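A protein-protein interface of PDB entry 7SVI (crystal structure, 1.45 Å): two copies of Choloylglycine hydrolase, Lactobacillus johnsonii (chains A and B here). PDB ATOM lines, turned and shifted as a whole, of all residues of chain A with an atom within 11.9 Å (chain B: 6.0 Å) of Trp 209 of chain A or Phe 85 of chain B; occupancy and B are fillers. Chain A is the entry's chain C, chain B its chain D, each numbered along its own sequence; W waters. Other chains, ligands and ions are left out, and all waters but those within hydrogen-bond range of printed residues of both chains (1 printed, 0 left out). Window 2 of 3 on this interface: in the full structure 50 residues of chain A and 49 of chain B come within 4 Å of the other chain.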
ATOM      1  N   ASP A 195      23.621 -22.690  35.288  1.00  0.00           N
ATOM      2  CA  ASP A 195      24.240 -22.505  33.983  1.00  0.00           C
ATOM      3  C   ASP A 195      24.310 -21.028  33.613  1.00  0.00           C
ATOM      4  O   ASP A 195      23.460 -20.219  33.996  1.00  0.00           O
ATOM      5  CB  ASP A 195      23.417 -23.208  32.902  1.00  0.00           C
ATOM      6  CG  ASP A 195      23.622 -24.707  32.883  1.00  0.00           C
ATOM      7  OD1 ASP A 195      24.603 -25.195  33.487  1.00  0.00           O
ATOM      8  OD2 ASP A 195      22.803 -25.393  32.240  1.00  0.00           O
ATOM      9  N   ALA A 196      25.342 -20.688  32.842  1.00  0.00           N
ATOM     10  CA  ALA A 196      25.442 -19.375  32.231  1.00  0.00           C
ATOM     11  C   ALA A 196      24.442 -19.268  31.085  1.00  0.00           C
ATOM     12  O   ALA A 196      23.836 -20.251  30.661  1.00  0.00           O
ATOM     13  CB  ALA A 196      26.848 -19.163  31.673  1.00  0.00           C
ATOM     14  N   THR A 197      24.273 -18.050  30.583  1.00  0.00           N
ATOM     15  CA  THR A 197      23.399 -17.770  29.454  1.00  0.00           C
ATOM     16  C   THR A 197      24.207 -17.138  28.323  1.00  0.00           C
ATOM     17  O   THR A 197      25.395 -16.837  28.467  1.00  0.00           O
ATOM     18  CB  THR A 197      22.254 -16.841  29.878  1.00  0.00           C
ATOM     19  OG1 THR A 197      22.796 -15.643  30.444  1.00  0.00           O
ATOM     20  CG2 THR A 197      21.394 -17.518  30.928  1.00  0.00           C
ATOM     21  N   ALA A 198      23.543 -16.938  27.185  1.00  0.00           N
ATOM     22  CA  ALA A 198      24.196 -16.329  26.035  1.00  0.00           C
ATOM     23  C   ALA A 198      24.703 -14.933  26.382  1.00  0.00           C
ATOM     24  O   ALA A 198      24.073 -14.194  27.146  1.00  0.00           O
ATOM     25  CB  ALA A 198      23.214 -16.255  24.865  1.00  0.00           C
ATOM     26  N   GLN A 199      25.857 -14.579  25.820  1.00  0.00           N
ATOM     27  CA  GLN A 199      26.545 -13.335  26.123  1.00  0.00           C
ATOM     28  C   GLN A 199      27.000 -12.689  24.824  1.00  0.00           C
ATOM     29  O   GLN A 199      26.957 -13.293  23.749  1.00  0.00           O
ATOM     30  CB  GLN A 199      27.758 -13.589  27.036  1.00  0.00           C
ATOM     31  CG  GLN A 199      27.381 -14.220  28.357  1.00  0.00           C
ATOM     32  CD  GLN A 199      28.568 -14.826  29.096  1.00  0.00           C
ATOM     33  OE1 GLN A 199      29.725 -14.682  28.693  1.00  0.00           O
ATOM     34  NE2 GLN A 199      28.276 -15.511  30.191  1.00  0.00           N
ATOM     35  N   TRP A 201      30.411 -10.707  23.603  1.00  0.00           N
ATOM     36  CA  TRP A 201      31.775 -10.282  23.902  1.00  0.00           C
ATOM     37  C   TRP A 201      32.152  -9.323  22.784  1.00  0.00           C
ATOM     38  O   TRP A 201      32.440  -9.756  21.670  1.00  0.00           O
ATOM     39  CB  TRP A 201      32.728 -11.475  23.932  1.00  0.00           C
ATOM     40  CG  TRP A 201      32.518 -12.453  25.072  1.00  0.00           C
ATOM     41  CD1 TRP A 201      31.348 -12.738  25.716  1.00  0.00           C
ATOM     42  CD2 TRP A 201      33.522 -13.279  25.682  1.00  0.00           C
ATOM     43  NE1 TRP A 201      31.564 -13.686  26.694  1.00  0.00           N
ATOM     44  CE2 TRP A 201      32.889 -14.035  26.690  1.00  0.00           C
ATOM     45  CE3 TRP A 201      34.893 -13.451  25.469  1.00  0.00           C
ATOM     46  CZ2 TRP A 201      33.583 -14.945  27.487  1.00  0.00           C
ATOM     47  CZ3 TRP A 201      35.582 -14.347  26.269  1.00  0.00           C
ATOM     48  CH2 TRP A 201      34.925 -15.087  27.261  1.00  0.00           C
ATOM     49  N   GLN A 204      30.346  -9.992  19.647  1.00  0.00           N
ATOM     50  CA  GLN A 204      30.349 -11.377  19.195  1.00  0.00           C
ATOM     51  C   GLN A 204      29.467 -12.207  20.122  1.00  0.00           C
ATOM     52  O   GLN A 204      29.672 -12.212  21.342  1.00  0.00           O
ATOM     53  CB  GLN A 204      31.774 -11.927  19.203  1.00  0.00           C
ATOM     54  CG  GLN A 204      31.865 -13.426  18.916  1.00  0.00           C
ATOM     55  CD  GLN A 204      31.441 -13.776  17.499  1.00  0.00           C
ATOM     56  OE1 GLN A 204      31.827 -13.108  16.546  1.00  0.00           O
ATOM     57  NE2 GLN A 204      30.630 -14.825  17.360  1.00  0.00           N
ATOM     58  N   LYS A 205      28.486 -12.902  19.552  1.00  0.00           N
ATOM     59  CA  LYS A 205      27.629 -13.766  20.356  1.00  0.00           C
ATOM     60  C   LYS A 205      28.443 -14.955  20.855  1.00  0.00           C
ATOM     61  O   LYS A 205      29.126 -15.626  20.074  1.00  0.00           O
ATOM     62  CB  LYS A 205      26.430 -14.235  19.530  1.00  0.00           C
ATOM     63  N   VAL A 206      28.401 -15.185  22.167  1.00  0.00           N
ATOM     64  CA  VAL A 206      29.101 -16.284  22.818  1.00  0.00           C
ATOM     65  C   VAL A 206      28.087 -16.976  23.717  1.00  0.00           C
ATOM     66  O   VAL A 206      27.544 -16.349  24.633  1.00  0.00           O
ATOM     67  CB  VAL A 206      30.284 -15.775  23.663  1.00  0.00           C
ATOM     68  CG1 VAL A 206      30.979 -16.937  24.370  1.00  0.00           C
ATOM     69  CG2 VAL A 206      31.271 -14.992  22.807  1.00  0.00           C
ATOM     70  N   ALA A 207      27.820 -18.254  23.457  1.00  0.00           N
ATOM     71  CA  ALA A 207      26.760 -18.942  24.186  1.00  0.00           C
ATOM     72  C   ALA A 207      27.206 -20.339  24.593  1.00  0.00           C
ATOM     73  O   ALA A 207      28.008 -20.964  23.889  1.00  0.00           O
ATOM     74  CB  ALA A 207      25.492 -19.054  23.328  1.00  0.00           C
ATOM     75  N   PRO A 208      26.693 -20.858  25.718  1.00  0.00           N
ATOM     76  CA  PRO A 208      27.023 -22.234  26.113  1.00  0.00           C
ATOM     77  C   PRO A 208      26.672 -23.230  25.022  1.00  0.00           C
ATOM     78  O   PRO A 208      25.694 -23.059  24.289  1.00  0.00           O
ATOM     79  CB  PRO A 208      26.142 -22.474  27.346  1.00  0.00           C
ATOM     80  CG  PRO A 208      25.890 -21.114  27.906  1.00  0.00           C
ATOM     81  CD  PRO A 208      25.826 -20.190  26.706  1.00  0.00           C
ATOM     82  N   TRP A 209      27.493 -24.277  24.919  1.00  0.00           N
ATOM     83  CA  TRP A 209      27.206 -25.403  24.035  1.00  0.00           C
ATOM     84  C   TRP A 209      26.447 -26.521  24.729  1.00  0.00           C
ATOM     85  O   TRP A 209      25.824 -27.342  24.048  1.00  0.00           O
ATOM     86  CB  TRP A 209      28.499 -25.978  23.455  1.00  0.00           C
ATOM     87  CG  TRP A 209      29.183 -25.007  22.580  1.00  0.00           C
ATOM     88  CD1 TRP A 209      30.338 -24.348  22.840  1.00  0.00           C
ATOM     89  CD2 TRP A 209      28.732 -24.550  21.294  1.00  0.00           C
ATOM     90  NE1 TRP A 209      30.653 -23.508  21.788  1.00  0.00           N
ATOM     91  CE2 TRP A 209      29.680 -23.618  20.830  1.00  0.00           C
ATOM     92  CE3 TRP A 209      27.624 -24.840  20.495  1.00  0.00           C
ATOM     93  CZ2 TRP A 209      29.555 -22.973  19.603  1.00  0.00           C
ATOM     94  CZ3 TRP A 209      27.508 -24.204  19.269  1.00  0.00           C
ATOM     95  CH2 TRP A 209      28.461 -23.279  18.839  1.00  0.00           C
ATOM     96  N   GLY A 210      26.503 -26.580  26.056  1.00  0.00           N
ATOM     97  CA  GLY A 210      25.783 -27.584  26.811  1.00  0.00           C
ATOM     98  C   GLY A 210      25.682 -27.109  28.243  1.00  0.00           C
ATOM     99  O   GLY A 210      26.148 -26.022  28.589  1.00  0.00           O
ATOM    100  N   VAL A 211      25.052 -27.930  29.076  1.00  0.00           N
ATOM    101  CA  VAL A 211      24.875 -27.551  30.475  1.00  0.00           C
ATOM    102  C   VAL A 211      26.180 -27.752  31.241  1.00  0.00           C
ATOM    103  O   VAL A 211      27.077 -28.484  30.820  1.00  0.00           O
ATOM    104  CB  VAL A 211      23.713 -28.326  31.121  1.00  0.00           C
ATOM    105  CG1 VAL A 211      22.422 -28.074  30.343  1.00  0.00           C
ATOM    106  CG2 VAL A 211      24.022 -29.811  31.162  1.00  0.00           C
ATOM    107  N   GLY A 212      26.275 -27.084  32.398  1.00  0.00           N
ATOM    108  CA  GLY A 212      27.403 -27.223  33.303  1.00  0.00           C
ATOM    109  C   GLY A 212      28.348 -26.038  33.344  1.00  0.00           C
ATOM    110  O   GLY A 212      29.335 -26.078  34.092  1.00  0.00           O
ATOM    111  N   THR A 213      28.069 -24.973  32.586  1.00  0.00           N
ATOM    112  CA  THR A 213      29.018 -23.873  32.435  1.00  0.00           C
ATOM    113  C   THR A 213      29.296 -23.128  33.739  1.00  0.00           C
ATOM    114  O   THR A 213      30.357 -22.503  33.861  1.00  0.00           O
ATOM    115  CB  THR A 213      28.518 -22.874  31.380  1.00  0.00           C
ATOM    116  OG1 THR A 213      27.133 -22.588  31.610  1.00  0.00           O
ATOM    117  CG2 THR A 213      28.711 -23.435  29.977  1.00  0.00           C
ATOM    118  N   GLY A 214      28.373 -23.170  34.707  1.00  0.00           N
ATOM    119  CA  GLY A 214      28.567 -22.427  35.944  1.00  0.00           C
ATOM    120  C   GLY A 214      29.686 -22.957  36.817  1.00  0.00           C
ATOM    121  O   GLY A 214      30.176 -22.230  37.687  1.00  0.00           O
ATOM    122  N   LEU A 216      32.697 -23.872  35.786  1.00  0.00           N
ATOM    123  CA  LEU A 216      34.003 -23.653  35.186  1.00  0.00           C
ATOM    124  C   LEU A 216      35.051 -23.504  36.277  1.00  0.00           C
ATOM    125  O   LEU A 216      34.846 -22.776  37.249  1.00  0.00           O
ATOM    126  CB  LEU A 216      33.943 -22.362  34.373  1.00  0.00           C
ATOM    127  CG  LEU A 216      35.251 -21.854  33.765  1.00  0.00           C
ATOM    128  CD1 LEU A 216      35.720 -22.749  32.644  1.00  0.00           C
ATOM    129  CD2 LEU A 216      35.063 -20.416  33.287  1.00  0.00           C
ATOM    130  N   PHE B  82      22.930 -33.304  21.273  1.00  0.00           N
ATOM    131  CA  PHE B  82      23.806 -32.558  20.368  1.00  0.00           C
ATOM    132  C   PHE B  82      23.143 -31.214  20.055  1.00  0.00           C
ATOM    133  O   PHE B  82      22.924 -30.867  18.891  1.00  0.00           O
ATOM    134  CB  PHE B  82      24.025 -33.399  19.108  1.00  0.00           C
ATOM    135  CG  PHE B  82      25.160 -32.961  18.231  1.00  0.00           C
ATOM    136  CD1 PHE B  82      26.346 -32.467  18.760  1.00  0.00           C
ATOM    137  CD2 PHE B  82      25.052 -33.094  16.847  1.00  0.00           C
ATOM    138  CE1 PHE B  82      27.387 -32.092  17.929  1.00  0.00           C
ATOM    139  CE2 PHE B  82      26.085 -32.723  16.005  1.00  0.00           C
ATOM    140  CZ  PHE B  82      27.264 -32.224  16.542  1.00  0.00           C
ATOM    141  N   PRO B  83      22.792 -30.437  21.081  1.00  0.00           N
ATOM    142  CA  PRO B  83      22.048 -29.195  20.841  1.00  0.00           C
ATOM    143  C   PRO B  83      22.929 -28.135  20.201  1.00  0.00           C
ATOM    144  O   PRO B  83      24.160 -28.190  20.251  1.00  0.00           O
ATOM    145  CB  PRO B  83      21.613 -28.763  22.244  1.00  0.00           C
ATOM    146  CG  PRO B  83      22.683 -29.311  23.144  1.00  0.00           C
ATOM    147  CD  PRO B  83      23.167 -30.586  22.500  1.00  0.00           C
ATOM    148  N   HIS B  84      22.270 -27.154  19.581  1.00  0.00           N
ATOM    149  CA  HIS B  84      22.921 -26.070  18.850  1.00  0.00           C
ATOM    150  C   HIS B  84      23.734 -26.561  17.663  1.00  0.00           C
ATOM    151  O   HIS B  84      24.550 -25.802  17.119  1.00  0.00           O
ATOM    152  CB  HIS B  84      23.775 -25.175  19.760  1.00  0.00           C
ATOM    153  CG  HIS B  84      23.258 -25.067  21.156  1.00  0.00           C
ATOM    154  ND1 HIS B  84      22.144 -24.322  21.480  1.00  0.00           N
ATOM    155  CD2 HIS B  84      23.693 -25.617  22.315  1.00  0.00           C
ATOM    156  CE1 HIS B  84      21.918 -24.416  22.777  1.00  0.00           C
ATOM    157  NE2 HIS B  84      22.845 -25.193  23.307  1.00  0.00           N
ATOM    158  N   PHE B  85      23.529 -27.806  17.231  1.00  0.00           N
ATOM    159  CA  PHE B  85      24.335 -28.379  16.164  1.00  0.00           C
ATOM    160  C   PHE B  85      23.511 -29.320  15.297  1.00  0.00           C
ATOM    161  O   PHE B  85      23.533 -29.218  14.065  1.00  0.00           O
ATOM    162  CB  PHE B  85      25.535 -29.136  16.742  1.00  0.00           C
ATOM    163  CG  PHE B  85      26.860 -28.466  16.477  1.00  0.00           C
ATOM    164  CD1 PHE B  85      27.551 -28.705  15.307  1.00  0.00           C
ATOM    165  CD2 PHE B  85      27.415 -27.601  17.412  1.00  0.00           C
ATOM    166  CE1 PHE B  85      28.770 -28.089  15.062  1.00  0.00           C
ATOM    167  CE2 PHE B  85      28.634 -26.985  17.162  1.00  0.00           C
ATOM    168  CZ  PHE B  85      29.305 -27.235  15.987  1.00  0.00           C
ATOM    169  N   ALA B  86      22.799 -30.251  15.925  1.00  0.00           N
ATOM    170  CA  ALA B  86      22.059 -31.245  15.158  1.00  0.00           C
ATOM    171  C   ALA B  86      21.035 -30.566  14.261  1.00  0.00           C
ATOM    172  O   ALA B  86      20.276 -29.699  14.703  1.00  0.00           O
ATOM    173  CB  ALA B  86      21.356 -32.224  16.095  1.00  0.00           C
ATOM    174  N   LYS B  87      21.024 -30.960  12.991  1.00  0.00           N
ATOM    175  CA  LYS B  87      20.055 -30.439  12.037  1.00  0.00           C
ATOM    176  C   LYS B  87      19.801 -31.519  10.999  1.00  0.00           C
ATOM    177  O   LYS B  87      20.741 -32.017  10.373  1.00  0.00           O
ATOM    178  CB  LYS B  87      20.581 -29.165  11.374  1.00  0.00           C
ATOM    179  CG  LYS B  87      19.676 -28.621  10.280  1.00  0.00           C
ATOM    180  CD  LYS B  87      18.424 -27.997  10.868  1.00  0.00           C
ATOM    181  CE  LYS B  87      17.764 -27.057   9.871  1.00  0.00           C
ATOM    182  NZ  LYS B  87      18.192 -27.359   8.475  1.00  0.00           N
ATOM    183  N   VAL B 156      25.101 -35.006  12.040  1.00  0.00           N
ATOM    184  CA  VAL B 156      24.501 -34.250  10.943  1.00  0.00           C
ATOM    185  C   VAL B 156      24.211 -32.857  11.481  1.00  0.00           C
ATOM    186  O   VAL B 156      23.384 -32.697  12.392  1.00  0.00           O
ATOM    187  CB  VAL B 156      23.225 -34.913  10.404  1.00  0.00           C
ATOM    188  CG1 VAL B 156      22.750 -34.183   9.139  1.00  0.00           C
ATOM    189  CG2 VAL B 156      23.489 -36.376  10.097  1.00  0.00           C
ATOM    190  N   SER B 157      24.901 -31.856  10.941  1.00  0.00           N
ATOM    191  CA  SER B 157      24.806 -30.496  11.438  1.00  0.00           C
ATOM    192  C   SER B 157      24.504 -29.536  10.301  1.00  0.00           C
ATOM    193  O   SER B 157      24.771 -29.813   9.129  1.00  0.00           O
ATOM    194  CB  SER B 157      26.121 -30.033  12.088  1.00  0.00           C
ATOM    195  OG  SER B 157      27.217 -30.293  11.240  1.00  0.00           O
ATOM    196  N   LYS B 158      23.956 -28.378  10.678  1.00  0.00           N
ATOM    197  CA  LYS B 158      23.865 -27.275   9.735  1.00  0.00           C
ATOM    198  C   LYS B 158      25.246 -26.821   9.280  1.00  0.00           C
ATOM    199  O   LYS B 158      25.417 -26.429   8.122  1.00  0.00           O
ATOM    200  CB  LYS B 158      23.092 -26.118  10.370  1.00  0.00           C
ATOM    201  N   GLN B 159      26.247 -26.895  10.165  1.00  0.00           N
ATOM    202  CA  GLN B 159      27.574 -26.373   9.846  1.00  0.00           C
ATOM    203  C   GLN B 159      28.332 -27.285   8.886  1.00  0.00           C
ATOM    204  O   GLN B 159      29.050 -26.801   8.003  1.00  0.00           O
ATOM    205  CB  GLN B 159      28.384 -26.186  11.132  1.00  0.00           C
ATOM    206  CG  GLN B 159      27.834 -25.135  12.092  1.00  0.00           C
ATOM    207  CD  GLN B 159      26.883 -25.711  13.121  1.00  0.00           C
ATOM    208  OE1 GLN B 159      26.208 -26.708  12.867  1.00  0.00           O
ATOM    209  NE2 GLN B 159      26.819 -25.080  14.297  1.00  0.00           N
ATOM    210  N   TYR B 160      28.202 -28.606   9.044  1.00  0.00           N
ATOM    211  CA  TYR B 160      29.048 -29.539   8.316  1.00  0.00           C
ATOM    212  C   TYR B 160      28.306 -30.613   7.529  1.00  0.00           C
ATOM    213  O   TYR B 160      28.965 -31.437   6.889  1.00  0.00           O
ATOM    214  CB  TYR B 160      30.057 -30.208   9.265  1.00  0.00           C
ATOM    215  CG  TYR B 160      30.846 -29.194  10.062  1.00  0.00           C
ATOM    216  CD1 TYR B 160      31.714 -28.321   9.428  1.00  0.00           C
ATOM    217  CD2 TYR B 160      30.711 -29.096  11.441  1.00  0.00           C
ATOM    218  CE1 TYR B 160      32.434 -27.380  10.135  1.00  0.00           C
ATOM    219  CE2 TYR B 160      31.430 -28.162  12.157  1.00  0.00           C
ATOM    220  CZ  TYR B 160      32.291 -27.306  11.498  1.00  0.00           C
ATOM    221  OH  TYR B 160      33.006 -26.363  12.213  1.00  0.00           O
ATOM    222  N   ASN B 174      28.752 -34.319  24.250  1.00  0.00           N
ATOM    223  CA  ASN B 174      27.731 -33.497  23.617  1.00  0.00           C
ATOM    224  C   ASN B 174      28.401 -32.403  22.787  1.00  0.00           C
ATOM    225  O   ASN B 174      29.512 -32.608  22.296  1.00  0.00           O
ATOM    226  CB  ASN B 174      26.774 -32.964  24.678  1.00  0.00           C
ATOM    227  CG  ASN B 174      26.280 -34.071  25.607  1.00  0.00           C
ATOM    228  OD1 ASN B 174      26.768 -34.229  26.734  1.00  0.00           O
ATOM    229  ND2 ASN B 174      25.336 -34.866  25.124  1.00  0.00           N
ATOM    230  N   SER B 175      27.763 -31.247  22.642  1.00  0.00           N
ATOM    231  CA  SER B 175      28.232 -30.267  21.669  1.00  0.00           C
ATOM    232  C   SER B 175      29.496 -29.558  22.180  1.00  0.00           C
ATOM    233  O   SER B 175      29.711 -29.444  23.394  1.00  0.00           O
ATOM    234  CB  SER B 175      27.127 -29.251  21.406  1.00  0.00           C
ATOM    235  OG  SER B 175      25.944 -29.907  20.935  1.00  0.00           O
ATOM    236  N   PRO B 176      30.345 -29.031  21.271  1.00  0.00           N
ATOM    237  CA  PRO B 176      30.192 -28.964  19.808  1.00  0.00           C
ATOM    238  C   PRO B 176      30.563 -30.250  19.066  1.00  0.00           C
ATOM    239  O   PRO B 176      30.494 -31.346  19.626  1.00  0.00           O
ATOM    240  CB  PRO B 176      31.125 -27.812  19.420  1.00  0.00           C
ATOM    241  CG  PRO B 176      32.228 -27.874  20.443  1.00  0.00           C
ATOM    242  CD  PRO B 176      31.537 -28.280  21.726  1.00  0.00           C
ATOM    243  N   ASP B 177      30.933 -30.107  17.792  1.00  0.00           N
ATOM    244  CA  ASP B 177      31.117 -31.252  16.922  1.00  0.00           C
ATOM    245  C   ASP B 177      32.364 -32.053  17.307  1.00  0.00           C
ATOM    246  O   ASP B 177      33.257 -31.592  18.028  1.00  0.00           O
ATOM    247  CB  ASP B 177      31.251 -30.785  15.476  1.00  0.00           C
ATOM    248  CG  ASP B 177      32.399 -29.815  15.302  1.00  0.00           C
ATOM    249  OD1 ASP B 177      32.253 -28.661  15.749  1.00  0.00           O
ATOM    250  OD2 ASP B 177      33.444 -30.223  14.762  1.00  0.00           O
ATOM    251  N   PRO B 224      30.398 -30.144  28.247  1.00  0.00           N
ATOM    252  CA  PRO B 224      30.697 -31.318  27.400  1.00  0.00           C
ATOM    253  C   PRO B 224      32.151 -31.422  26.977  1.00  0.00           C
ATOM    254  O   PRO B 224      32.717 -32.521  26.977  1.00  0.00           O
ATOM    255  CB  PRO B 224      29.757 -31.138  26.195  1.00  0.00           C
ATOM    256  CG  PRO B 224      28.606 -30.365  26.739  1.00  0.00           C
ATOM    257  CD  PRO B 224      29.214 -29.407  27.761  1.00  0.00           C
HETATM  258  O   HOH W   1      25.712 -30.004  24.411  1.00  0.00           O
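Water W1 lies within hydrogen-bond range of the backbone carbonyl oxygen (O) of Trp 209 of chain A (2.7 Å) and the backbone NH (N) of Ser 175 of chain B (3.0 Å).
Among the printed residues, merely in contact across the chains: Pro 208 of chain A with His 84 of chain B (3.7 Å), Trp 209 of chain A with Pro 83 of chain B (3.8 Å), Trp 209 of chain A with His 84 of chain B (3.2 Å), Trp 209 of chain A with Phe 85 of chain B (3.7 Å), Trp 209 of chain A with Ser 175 of chain B (3.5 Å), Gly 210 of chain A with Pro 224 of chain B (3.96 Å) and Val 211 of chain A with Pro 224 of chain B (3.8 Å).
OG of Ser 175 of chain B lies within hydrogen-bond range of O of Pro 83 of chain B (2.6 Å).
Hydrophobic or aromatic side chains of chain B within 4 Å of the printed part of chain A: Pro 83, His 84, Phe 85 and Pro 224. Of the 18 printed residues of chain A, 4 touch a printed residue of chain B. Printed residues of chain A that touch a printed residue of chain B: Pro 208, Trp 209, Gly 210 and Val 211. Along chain A the printed residues that touch a printed residue of chain B span positions 208 to 211. Among the printed residues, no Asp or Glu carboxylate lies within 4 Å of a Lys or Arg side-chain nitrogen of the other chain.
Of the printed residues of chain B, Pro 208 of chain A touches His 84. Trp 209 of chain A touches just these residues of chain B: Pro 83 (3.8 Å), His 84 (3.2 Å), Phe 85 (3.7 Å) and Ser 175 (3.5 Å). Of the printed residues of chain B, Gly 210 of chain A touches Pro 224. Printed residues of chain B within 4 Å of Val 211 of chain A: Pro 224. Pro 83 of chain B touches one residue of chain A. His 84 of chain B touches just these residues of chain A: Pro 208 and Trp 209. Phe 85 of chain B touches just one residue of chain A: Trp 209. Ala 86 of chain B touches none of the printed residues of chain A. No residue of chain A comes within 4 Å of Lys 158 of chain B. No residue of chain A comes within 4 Å of Gln 159 of chain B. No residue of chain A comes within 4 Å of Asn 174 of chain B. No residue of chain A comes within 4 Å of Pro 176 of chain B. Asp 177 of chain B touches none of the printed residues of chain A. Printed residues of chain A within 4 Å of Pro 224 of chain B: Gly 210 (3.96 Å) and Val 211 (3.8 Å). The nearest printed residue of chain B that does not touch Val 211 of chain A is Pro 83 of chain B (6.5 Å).
No position is printed for both chains.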
